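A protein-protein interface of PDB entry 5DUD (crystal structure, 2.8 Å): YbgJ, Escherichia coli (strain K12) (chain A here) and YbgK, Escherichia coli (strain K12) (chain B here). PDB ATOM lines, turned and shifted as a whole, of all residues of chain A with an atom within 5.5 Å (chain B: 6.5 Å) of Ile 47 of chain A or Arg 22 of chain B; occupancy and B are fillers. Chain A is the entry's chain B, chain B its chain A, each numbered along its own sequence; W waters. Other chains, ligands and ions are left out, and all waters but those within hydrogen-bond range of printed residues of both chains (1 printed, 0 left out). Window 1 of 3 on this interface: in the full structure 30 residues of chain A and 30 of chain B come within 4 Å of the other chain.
OE2 of Glu 45 of chain A sits at hydrogen-bond distance from N of Gly 20 of chain B (2.6 Å). N of Phe 21 of chain B sits at hydrogen-bond distance from OE1 of Glu 45 of chain A (3.3 Å). The side-chain carboxylate of Glu 45 of chain A is in hydrogen-bond range of the backbone NH of Arg 22 of chain B, 2.9 Å away.
O of Phe 21 of chain B is in hydrogen-bond range of N of Ile 26 of chain B (3.2 Å). O of Glu 45 of chain A sits at hydrogen-bond distance from N of Ile 56 of chain A. The backbone NH (N) of Ile 47 of chain A sits at hydrogen-bond distance from the backbone carbonyl oxygen (O) of Thr 54 of chain A (2.8 Å).
His 19 of chain B touches Glu 45 of chain A (C to OE2, 3.6 Å). Ala 46 of chain A touches Gln 23 of chain B. Arg 22 of chain B touches Ile 47 of chain A (CB to CD1, 3.6 Å). His 227 of chain B touches Asn 52 of chain A (CA to OD1, 3.8 Å). Thr 54 of chain A touches Gly 228 of chain B. Gln 23 of chain B touches Leu 130 of chain A. Leu 130 of chain A touches Ser 24 of chain B.
Of the printed residues of chain B, Ile 47 of chain A touches Arg 22 (3.6 Å). Arg 22 of chain B touches two residues of chain A. Printed residues of chain A within 4 Å of Phe 21 of chain B: Glu 45 (3.3 Å). Of the printed residues of chain B, Glu 45 of chain A touches His 19 (3.6 Å), Gly 20 (2.6 Å), Phe 21 (3.3 Å) and Arg 22 (2.9 Å). Printed residues of chain A within 4 Å of Gly 228 of chain B: Thr 54 (3.7 Å). Pro 231 of chain B touches none of the printed residues of chain A.
Of the 19 printed residues of chain B, 8 touch a printed residue of chain A. Hydrophobic or aromatic side chains of chain B within 4 Å of the printed part of chain A: His 227. Printed residues of chain A that touch a printed residue of chain B: Glu 45, Ala 46, Ile 47, Asn 52, Thr 54 and Leu 130. Among the printed residues, 10 pairs touch across the chains.
Water W1 lies within hydrogen-bond range of OG1 of Thr 54 of chain A (2.7 Å), OD1 of Asn 52 of chain A (2.7 Å), N of Gly 228 of chain B (2.9 Å) and O of Ile 47 of chain A (2.9 Å).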
ATOM      1  N   GLU A  45     -14.839   4.705 -22.959  1.00  0.00           N
ATOM      2  CA  GLU A  45     -16.203   4.310 -23.343  1.00  0.00           C
ATOM      3  C   GLU A  45     -17.156   5.490 -23.222  1.00  0.00           C
ATOM      4  O   GLU A  45     -16.867   6.438 -22.494  1.00  0.00           O
ATOM      5  CB  GLU A  45     -16.747   3.163 -22.456  1.00  0.00           C
ATOM      6  CG  GLU A  45     -15.818   1.990 -22.153  1.00  0.00           C
ATOM      7  CD  GLU A  45     -15.877   0.782 -23.065  1.00  0.00           C
ATOM      8  OE1 GLU A  45     -16.701   0.766 -24.007  1.00  0.00           O
ATOM      9  OE2 GLU A  45     -15.100  -0.169 -22.820  1.00  0.00           O
ATOM     10  N   ALA A  46     -18.307   5.402 -23.912  1.00  0.00           N
ATOM     11  CA  ALA A  46     -19.396   6.378 -23.863  1.00  0.00           C
ATOM     12  C   ALA A  46     -20.702   5.589 -23.940  1.00  0.00           C
ATOM     13  O   ALA A  46     -21.109   5.161 -25.024  1.00  0.00           O
ATOM     14  CB  ALA A  46     -19.276   7.385 -24.999  1.00  0.00           C
ATOM     15  N   ILE A  47     -21.296   5.302 -22.776  1.00  0.00           N
ATOM     16  CA  ILE A  47     -22.484   4.452 -22.667  1.00  0.00           C
ATOM     17  C   ILE A  47     -23.784   5.275 -22.525  1.00  0.00           C
ATOM     18  O   ILE A  47     -24.061   5.783 -21.435  1.00  0.00           O
ATOM     19  CB  ILE A  47     -22.328   3.488 -21.453  1.00  0.00           C
ATOM     20  CG1 ILE A  47     -20.966   2.743 -21.471  1.00  0.00           C
ATOM     21  CG2 ILE A  47     -23.492   2.487 -21.397  1.00  0.00           C
ATOM     22  CD1 ILE A  47     -20.500   2.299 -20.107  1.00  0.00           C
ATOM     23  N   PRO A  48     -24.628   5.369 -23.574  1.00  0.00           N
ATOM     24  CA  PRO A  48     -25.904   6.079 -23.411  1.00  0.00           C
ATOM     25  C   PRO A  48     -26.927   5.221 -22.676  1.00  0.00           C
ATOM     26  O   PRO A  48     -26.793   3.998 -22.638  1.00  0.00           O
ATOM     27  CB  PRO A  48     -26.328   6.350 -24.848  1.00  0.00           C
ATOM     28  CG  PRO A  48     -25.800   5.197 -25.604  1.00  0.00           C
ATOM     29  CD  PRO A  48     -24.507   4.806 -24.934  1.00  0.00           C
ATOM     30  N   GLY A  49     -27.928   5.874 -22.098  1.00  0.00           N
ATOM     31  CA  GLY A  49     -29.009   5.217 -21.377  1.00  0.00           C
ATOM     32  C   GLY A  49     -30.331   5.834 -21.769  1.00  0.00           C
ATOM     33  O   GLY A  49     -30.584   6.040 -22.956  1.00  0.00           O
ATOM     34  N   ASN A  52     -29.666  10.100 -20.825  1.00  0.00           N
ATOM     35  CA  ASN A  52     -28.444  10.247 -20.046  1.00  0.00           C
ATOM     36  C   ASN A  52     -27.302   9.522 -20.743  1.00  0.00           C
ATOM     37  O   ASN A  52     -27.537   8.552 -21.461  1.00  0.00           O
ATOM     38  CB  ASN A  52     -28.610   9.752 -18.592  1.00  0.00           C
ATOM     39  CG  ASN A  52     -28.950   8.283 -18.430  1.00  0.00           C
ATOM     40  OD1 ASN A  52     -28.180   7.397 -18.799  1.00  0.00           O
ATOM     41  ND2 ASN A  52     -30.076   7.983 -17.801  1.00  0.00           N
ATOM     42  N   ILE A  53     -26.070   9.985 -20.528  1.00  0.00           N
ATOM     43  CA  ILE A  53     -24.882   9.364 -21.117  1.00  0.00           C
ATOM     44  C   ILE A  53     -23.788   9.301 -20.060  1.00  0.00           C
ATOM     45  O   ILE A  53     -23.592  10.268 -19.327  1.00  0.00           O
ATOM     46  CB  ILE A  53     -24.421  10.090 -22.415  1.00  0.00           C
ATOM     47  CG1 ILE A  53     -23.243   9.355 -23.082  1.00  0.00           C
ATOM     48  CG2 ILE A  53     -24.097  11.573 -22.176  1.00  0.00           C
ATOM     49  CD1 ILE A  53     -23.009   9.738 -24.545  1.00  0.00           C
ATOM     50  N   THR A  54     -23.118   8.137 -19.958  1.00  0.00           N
ATOM     51  CA  THR A  54     -22.036   7.880 -19.013  1.00  0.00           C
ATOM     52  C   THR A  54     -20.756   7.830 -19.814  1.00  0.00           C
ATOM     53  O   THR A  54     -20.605   6.947 -20.659  1.00  0.00           O
ATOM     54  CB  THR A  54     -22.297   6.570 -18.249  1.00  0.00           C
ATOM     55  OG1 THR A  54     -23.580   6.653 -17.638  1.00  0.00           O
ATOM     56  CG2 THR A  54     -21.261   6.286 -17.171  1.00  0.00           C
ATOM     57  N   VAL A  55     -19.830   8.761 -19.543  1.00  0.00           N
ATOM     58  CA  VAL A  55     -18.561   8.854 -20.253  1.00  0.00           C
ATOM     59  C   VAL A  55     -17.416   8.443 -19.328  1.00  0.00           C
ATOM     60  O   VAL A  55     -17.069   9.203 -18.430  1.00  0.00           O
ATOM     61  CB  VAL A  55     -18.345  10.291 -20.802  1.00  0.00           C
ATOM     62  CG1 VAL A  55     -17.203  10.311 -21.811  1.00  0.00           C
ATOM     63  CG2 VAL A  55     -19.623  10.848 -21.424  1.00  0.00           C
ATOM     64  N   ILE A  56     -16.834   7.251 -19.536  1.00  0.00           N
ATOM     65  CA  ILE A  56     -15.706   6.786 -18.727  1.00  0.00           C
ATOM     66  C   ILE A  56     -14.454   7.409 -19.337  1.00  0.00           C
ATOM     67  O   ILE A  56     -14.374   7.514 -20.557  1.00  0.00           O
ATOM     68  CB  ILE A  56     -15.649   5.242 -18.629  1.00  0.00           C
ATOM     69  N   LEU A 130     -28.251   0.326 -25.898  1.00  0.00           N
ATOM     70  CA  LEU A 130     -27.952  -1.091 -25.756  1.00  0.00           C
ATOM     71  C   LEU A 130     -27.404  -1.337 -24.361  1.00  0.00           C
ATOM     72  O   LEU A 130     -26.575  -0.560 -23.889  1.00  0.00           O
ATOM     73  CB  LEU A 130     -26.926  -1.534 -26.814  1.00  0.00           C
ATOM     74  CG  LEU A 130     -27.278  -1.227 -28.266  1.00  0.00           C
ATOM     75  CD1 LEU A 130     -26.031  -1.138 -29.118  1.00  0.00           C
ATOM     76  CD2 LEU A 130     -28.193  -2.288 -28.831  1.00  0.00           C
ATOM     77  N   ARG B  18     -12.001  -7.050 -21.903  1.00  0.00           N
ATOM     78  CA  ARG B  18     -12.597  -6.837 -23.219  1.00  0.00           C
ATOM     79  C   ARG B  18     -13.181  -5.409 -23.264  1.00  0.00           C
ATOM     80  O   ARG B  18     -14.383  -5.224 -23.116  1.00  0.00           O
ATOM     81  CB  ARG B  18     -13.656  -7.929 -23.461  1.00  0.00           C
ATOM     82  CG  ARG B  18     -14.191  -7.980 -24.880  1.00  0.00           C
ATOM     83  CD  ARG B  18     -15.001  -9.227 -25.191  1.00  0.00           C
ATOM     84  NE  ARG B  18     -14.161 -10.428 -25.276  1.00  0.00           N
ATOM     85  CZ  ARG B  18     -13.953 -11.322 -24.306  1.00  0.00           C
ATOM     86  NH1 ARG B  18     -14.532 -11.177 -23.115  1.00  0.00           N
ATOM     87  NH2 ARG B  18     -13.161 -12.366 -24.516  1.00  0.00           N
ATOM     88  N   HIS B  19     -12.307  -4.401 -23.441  1.00  0.00           N
ATOM     89  CA  HIS B  19     -12.683  -2.980 -23.429  1.00  0.00           C
ATOM     90  C   HIS B  19     -13.172  -2.482 -24.805  1.00  0.00           C
ATOM     91  O   HIS B  19     -12.989  -3.151 -25.817  1.00  0.00           O
ATOM     92  CB  HIS B  19     -11.498  -2.120 -22.949  1.00  0.00           C
ATOM     93  CG  HIS B  19     -10.935  -2.537 -21.620  1.00  0.00           C
ATOM     94  ND1 HIS B  19      -9.713  -3.178 -21.523  1.00  0.00           N
ATOM     95  CD2 HIS B  19     -11.462  -2.415 -20.379  1.00  0.00           C
ATOM     96  CE1 HIS B  19      -9.524  -3.408 -20.234  1.00  0.00           C
ATOM     97  NE2 HIS B  19     -10.546  -2.956 -19.506  1.00  0.00           N
ATOM     98  N   GLY B  20     -13.759  -1.279 -24.807  1.00  0.00           N
ATOM     99  CA  GLY B  20     -14.329  -0.613 -25.975  1.00  0.00           C
ATOM    100  C   GLY B  20     -15.739  -1.022 -26.355  1.00  0.00           C
ATOM    101  O   GLY B  20     -16.288  -0.425 -27.284  1.00  0.00           O
ATOM    102  N   PHE B  21     -16.354  -2.020 -25.686  1.00  0.00           N
ATOM    103  CA  PHE B  21     -17.688  -2.478 -26.071  1.00  0.00           C
ATOM    104  C   PHE B  21     -18.737  -2.413 -24.947  1.00  0.00           C
ATOM    105  O   PHE B  21     -19.722  -3.130 -25.016  1.00  0.00           O
ATOM    106  CB  PHE B  21     -17.629  -3.912 -26.641  1.00  0.00           C
ATOM    107  CG  PHE B  21     -16.410  -4.207 -27.487  1.00  0.00           C
ATOM    108  CD1 PHE B  21     -16.330  -3.770 -28.800  1.00  0.00           C
ATOM    109  CD2 PHE B  21     -15.320  -4.868 -26.953  1.00  0.00           C
ATOM    110  CE1 PHE B  21     -15.200  -4.036 -29.574  1.00  0.00           C
ATOM    111  CE2 PHE B  21     -14.199  -5.140 -27.727  1.00  0.00           C
ATOM    112  CZ  PHE B  21     -14.136  -4.718 -29.029  1.00  0.00           C
ATOM    113  N   ARG B  22     -18.572  -1.504 -23.970  1.00  0.00           N
ATOM    114  CA  ARG B  22     -19.566  -1.324 -22.902  1.00  0.00           C
ATOM    115  C   ARG B  22     -20.837  -0.663 -23.443  1.00  0.00           C
ATOM    116  O   ARG B  22     -21.912  -0.850 -22.873  1.00  0.00           O
ATOM    117  CB  ARG B  22     -19.021  -0.484 -21.748  1.00  0.00           C
ATOM    118  CG  ARG B  22     -18.135  -1.248 -20.768  1.00  0.00           C
ATOM    119  CD  ARG B  22     -18.672  -1.109 -19.348  1.00  0.00           C
ATOM    120  NE  ARG B  22     -17.733  -1.577 -18.330  1.00  0.00           N
ATOM    121  CZ  ARG B  22     -16.676  -0.898 -17.881  1.00  0.00           C
ATOM    122  NH1 ARG B  22     -16.383   0.302 -18.378  1.00  0.00           N
ATOM    123  NH2 ARG B  22     -15.896  -1.418 -16.942  1.00  0.00           N
ATOM    124  N   GLN B  23     -20.704   0.119 -24.542  1.00  0.00           N
ATOM    125  CA  GLN B  23     -21.820   0.800 -25.212  1.00  0.00           C
ATOM    126  C   GLN B  23     -22.770  -0.198 -25.914  1.00  0.00           C
ATOM    127  O   GLN B  23     -23.922   0.148 -26.164  1.00  0.00           O
ATOM    128  CB  GLN B  23     -21.287   1.809 -26.245  1.00  0.00           C
ATOM    129  N   SER B  24     -22.292  -1.428 -26.231  1.00  0.00           N
ATOM    130  CA  SER B  24     -23.081  -2.475 -26.883  1.00  0.00           C
ATOM    131  C   SER B  24     -23.498  -3.630 -25.926  1.00  0.00           C
ATOM    132  O   SER B  24     -23.901  -4.687 -26.408  1.00  0.00           O
ATOM    133  CB  SER B  24     -22.297  -3.045 -28.057  1.00  0.00           C
ATOM    134  OG  SER B  24     -21.780  -2.023 -28.895  1.00  0.00           O
ATOM    135  N   GLY B  25     -23.449  -3.408 -24.610  1.00  0.00           N
ATOM    136  CA  GLY B  25     -23.879  -4.388 -23.618  1.00  0.00           C
ATOM    137  C   GLY B  25     -22.916  -5.507 -23.285  1.00  0.00           C
ATOM    138  O   GLY B  25     -23.336  -6.492 -22.677  1.00  0.00           O
ATOM    139  N   ILE B  26     -21.621  -5.364 -23.629  1.00  0.00           N
ATOM    140  CA  ILE B  26     -20.607  -6.384 -23.342  1.00  0.00           C
ATOM    141  C   ILE B  26     -19.815  -5.972 -22.101  1.00  0.00           C
ATOM    142  O   ILE B  26     -19.222  -4.893 -22.080  1.00  0.00           O
ATOM    143  CB  ILE B  26     -19.677  -6.619 -24.577  1.00  0.00           C
ATOM    144  CG1 ILE B  26     -20.443  -7.377 -25.675  1.00  0.00           C
ATOM    145  CG2 ILE B  26     -18.375  -7.371 -24.188  1.00  0.00           C
ATOM    146  CD1 ILE B  26     -19.973  -7.140 -27.162  1.00  0.00           C
ATOM    147  N   SER B  27     -19.770  -6.855 -21.090  1.00  0.00           N
ATOM    148  CA  SER B  27     -19.014  -6.631 -19.857  1.00  0.00           C
ATOM    149  C   SER B  27     -17.525  -6.801 -20.152  1.00  0.00           C
ATOM    150  O   SER B  27     -17.175  -7.652 -20.969  1.00  0.00           O
ATOM    151  CB  SER B  27     -19.469  -7.609 -18.779  1.00  0.00           C
ATOM    152  OG  SER B  27     -20.885  -7.709 -18.729  1.00  0.00           O
ATOM    153  N   HIS B  28     -16.655  -5.972 -19.541  1.00  0.00           N
ATOM    154  CA  HIS B  28     -15.214  -6.018 -19.805  1.00  0.00           C
ATOM    155  C   HIS B  28     -14.558  -7.284 -19.219  1.00  0.00           C
ATOM    156  O   HIS B  28     -13.558  -7.743 -19.772  1.00  0.00           O
ATOM    157  CB  HIS B  28     -14.502  -4.745 -19.296  1.00  0.00           C
ATOM    158  CG  HIS B  28     -14.169  -4.745 -17.836  1.00  0.00           C
ATOM    159  ND1 HIS B  28     -12.857  -4.744 -17.398  1.00  0.00           N
ATOM    160  CD2 HIS B  28     -14.985  -4.753 -16.758  1.00  0.00           C
ATOM    161  CE1 HIS B  28     -12.912  -4.729 -16.078  1.00  0.00           C
ATOM    162  NE2 HIS B  28     -14.174  -4.749 -15.646  1.00  0.00           N
ATOM    163  N   HIS B 227     -29.504   3.589 -16.489  1.00  0.00           N
ATOM    164  CA  HIS B 227     -28.250   4.330 -16.635  1.00  0.00           C
ATOM    165  C   HIS B 227     -27.068   3.397 -16.701  1.00  0.00           C
ATOM    166  O   HIS B 227     -27.098   2.320 -16.111  1.00  0.00           O
ATOM    167  CB  HIS B 227     -28.055   5.326 -15.462  1.00  0.00           C
ATOM    168  CG  HIS B 227     -28.355   4.756 -14.109  1.00  0.00           C
ATOM    169  ND1 HIS B 227     -27.580   3.753 -13.556  1.00  0.00           N
ATOM    170  CD2 HIS B 227     -29.350   5.061 -13.245  1.00  0.00           C
ATOM    171  CE1 HIS B 227     -28.124   3.480 -12.382  1.00  0.00           C
ATOM    172  NE2 HIS B 227     -29.188   4.249 -12.149  1.00  0.00           N
ATOM    173  N   GLY B 228     -26.022   3.841 -17.393  1.00  0.00           N
ATOM    174  CA  GLY B 228     -24.781   3.093 -17.533  1.00  0.00           C
ATOM    175  C   GLY B 228     -24.133   2.835 -16.189  1.00  0.00           C
ATOM    176  O   GLY B 228     -24.149   3.713 -15.321  1.00  0.00           O
ATOM    177  N   LEU B 229     -23.597   1.615 -16.002  1.00  0.00           N
ATOM    178  CA  LEU B 229     -22.946   1.158 -14.774  1.00  0.00           C
ATOM    179  C   LEU B 229     -21.490   0.790 -15.031  1.00  0.00           C
ATOM    180  O   LEU B 229     -21.083   0.626 -16.181  1.00  0.00           O
ATOM    181  CB  LEU B 229     -23.667  -0.088 -14.215  1.00  0.00           C
ATOM    182  CG  LEU B 229     -25.180  -0.026 -14.082  1.00  0.00           C
ATOM    183  CD1 LEU B 229     -25.721  -1.351 -13.549  1.00  0.00           C
ATOM    184  CD2 LEU B 229     -25.602   1.116 -13.176  1.00  0.00           C
ATOM    185  N   LEU B 230     -20.721   0.609 -13.948  1.00  0.00           N
ATOM    186  CA  LEU B 230     -19.320   0.183 -14.009  1.00  0.00           C
ATOM    187  C   LEU B 230     -18.966  -0.625 -12.759  1.00  0.00           C
ATOM    188  O   LEU B 230     -19.644  -0.481 -11.741  1.00  0.00           O
ATOM    189  CB  LEU B 230     -18.366   1.381 -14.181  1.00  0.00           C
ATOM    190  CG  LEU B 230     -18.457   2.569 -13.204  1.00  0.00           C
ATOM    191  CD1 LEU B 230     -17.543   2.377 -11.996  1.00  0.00           C
ATOM    192  CD2 LEU B 230     -18.063   3.864 -13.900  1.00  0.00           C
ATOM    193  N   PRO B 231     -17.927  -1.487 -12.800  1.00  0.00           N
ATOM    194  CA  PRO B 231     -17.570  -2.261 -11.595  1.00  0.00           C
ATOM    195  C   PRO B 231     -17.252  -1.372 -10.396  1.00  0.00           C
ATOM    196  O   PRO B 231     -16.638  -0.322 -10.565  1.00  0.00           O
ATOM    197  CB  PRO B 231     -16.330  -3.049 -12.029  1.00  0.00           C
ATOM    198  CG  PRO B 231     -16.392  -3.090 -13.499  1.00  0.00           C
ATOM    199  CD  PRO B 231     -17.026  -1.810 -13.923  1.00  0.00           C
ATOM    200  N   ASN B 247     -16.754  -7.305 -12.273  1.00  0.00           N
ATOM    201  CA  ASN B 247     -16.353  -7.198 -13.681  1.00  0.00           C
ATOM    202  C   ASN B 247     -17.378  -7.743 -14.701  1.00  0.00           C
ATOM    203  O   ASN B 247     -17.577  -7.087 -15.718  1.00  0.00           O
ATOM    204  CB  ASN B 247     -15.005  -7.878 -13.906  1.00  0.00           C
ATOM    205  CG  ASN B 247     -13.876  -7.324 -13.062  1.00  0.00           C
ATOM    206  OD1 ASN B 247     -14.081  -6.838 -11.945  1.00  0.00           O
ATOM    207  ND2 ASN B 247     -12.645  -7.432 -13.544  1.00  0.00           N
ATOM    208  N   THR B 251     -24.136  -3.815 -17.919  1.00  0.00           N
ATOM    209  CA  THR B 251     -23.667  -2.479 -18.284  1.00  0.00           C
ATOM    210  C   THR B 251     -24.717  -1.393 -17.954  1.00  0.00           C
ATOM    211  O   THR B 251     -24.318  -0.261 -17.706  1.00  0.00           O
ATOM    212  CB  THR B 251     -23.294  -2.412 -19.757  1.00  0.00           C
ATOM    213  OG1 THR B 251     -24.449  -2.688 -20.542  1.00  0.00           O
ATOM    214  CG2 THR B 251     -22.166  -3.369 -20.116  1.00  0.00           C
ATOM    215  N   THR B 252     -26.037  -1.728 -17.963  1.00  0.00           N
ATOM    216  CA  THR B 252     -27.130  -0.785 -17.660  1.00  0.00           C
ATOM    217  C   THR B 252     -28.020  -1.314 -16.527  1.00  0.00           C
ATOM    218  O   THR B 252     -28.240  -2.518 -16.438  1.00  0.00           O
ATOM    219  CB  THR B 252     -27.987  -0.537 -18.908  1.00  0.00           C
ATOM    220  OG1 THR B 252     -28.420  -1.789 -19.433  1.00  0.00           O
ATOM    221  CG2 THR B 252     -27.253   0.273 -19.972  1.00  0.00           C
HETATM  222  O   HOH W   1     -25.769   6.180 -19.110  1.00  0.00           O
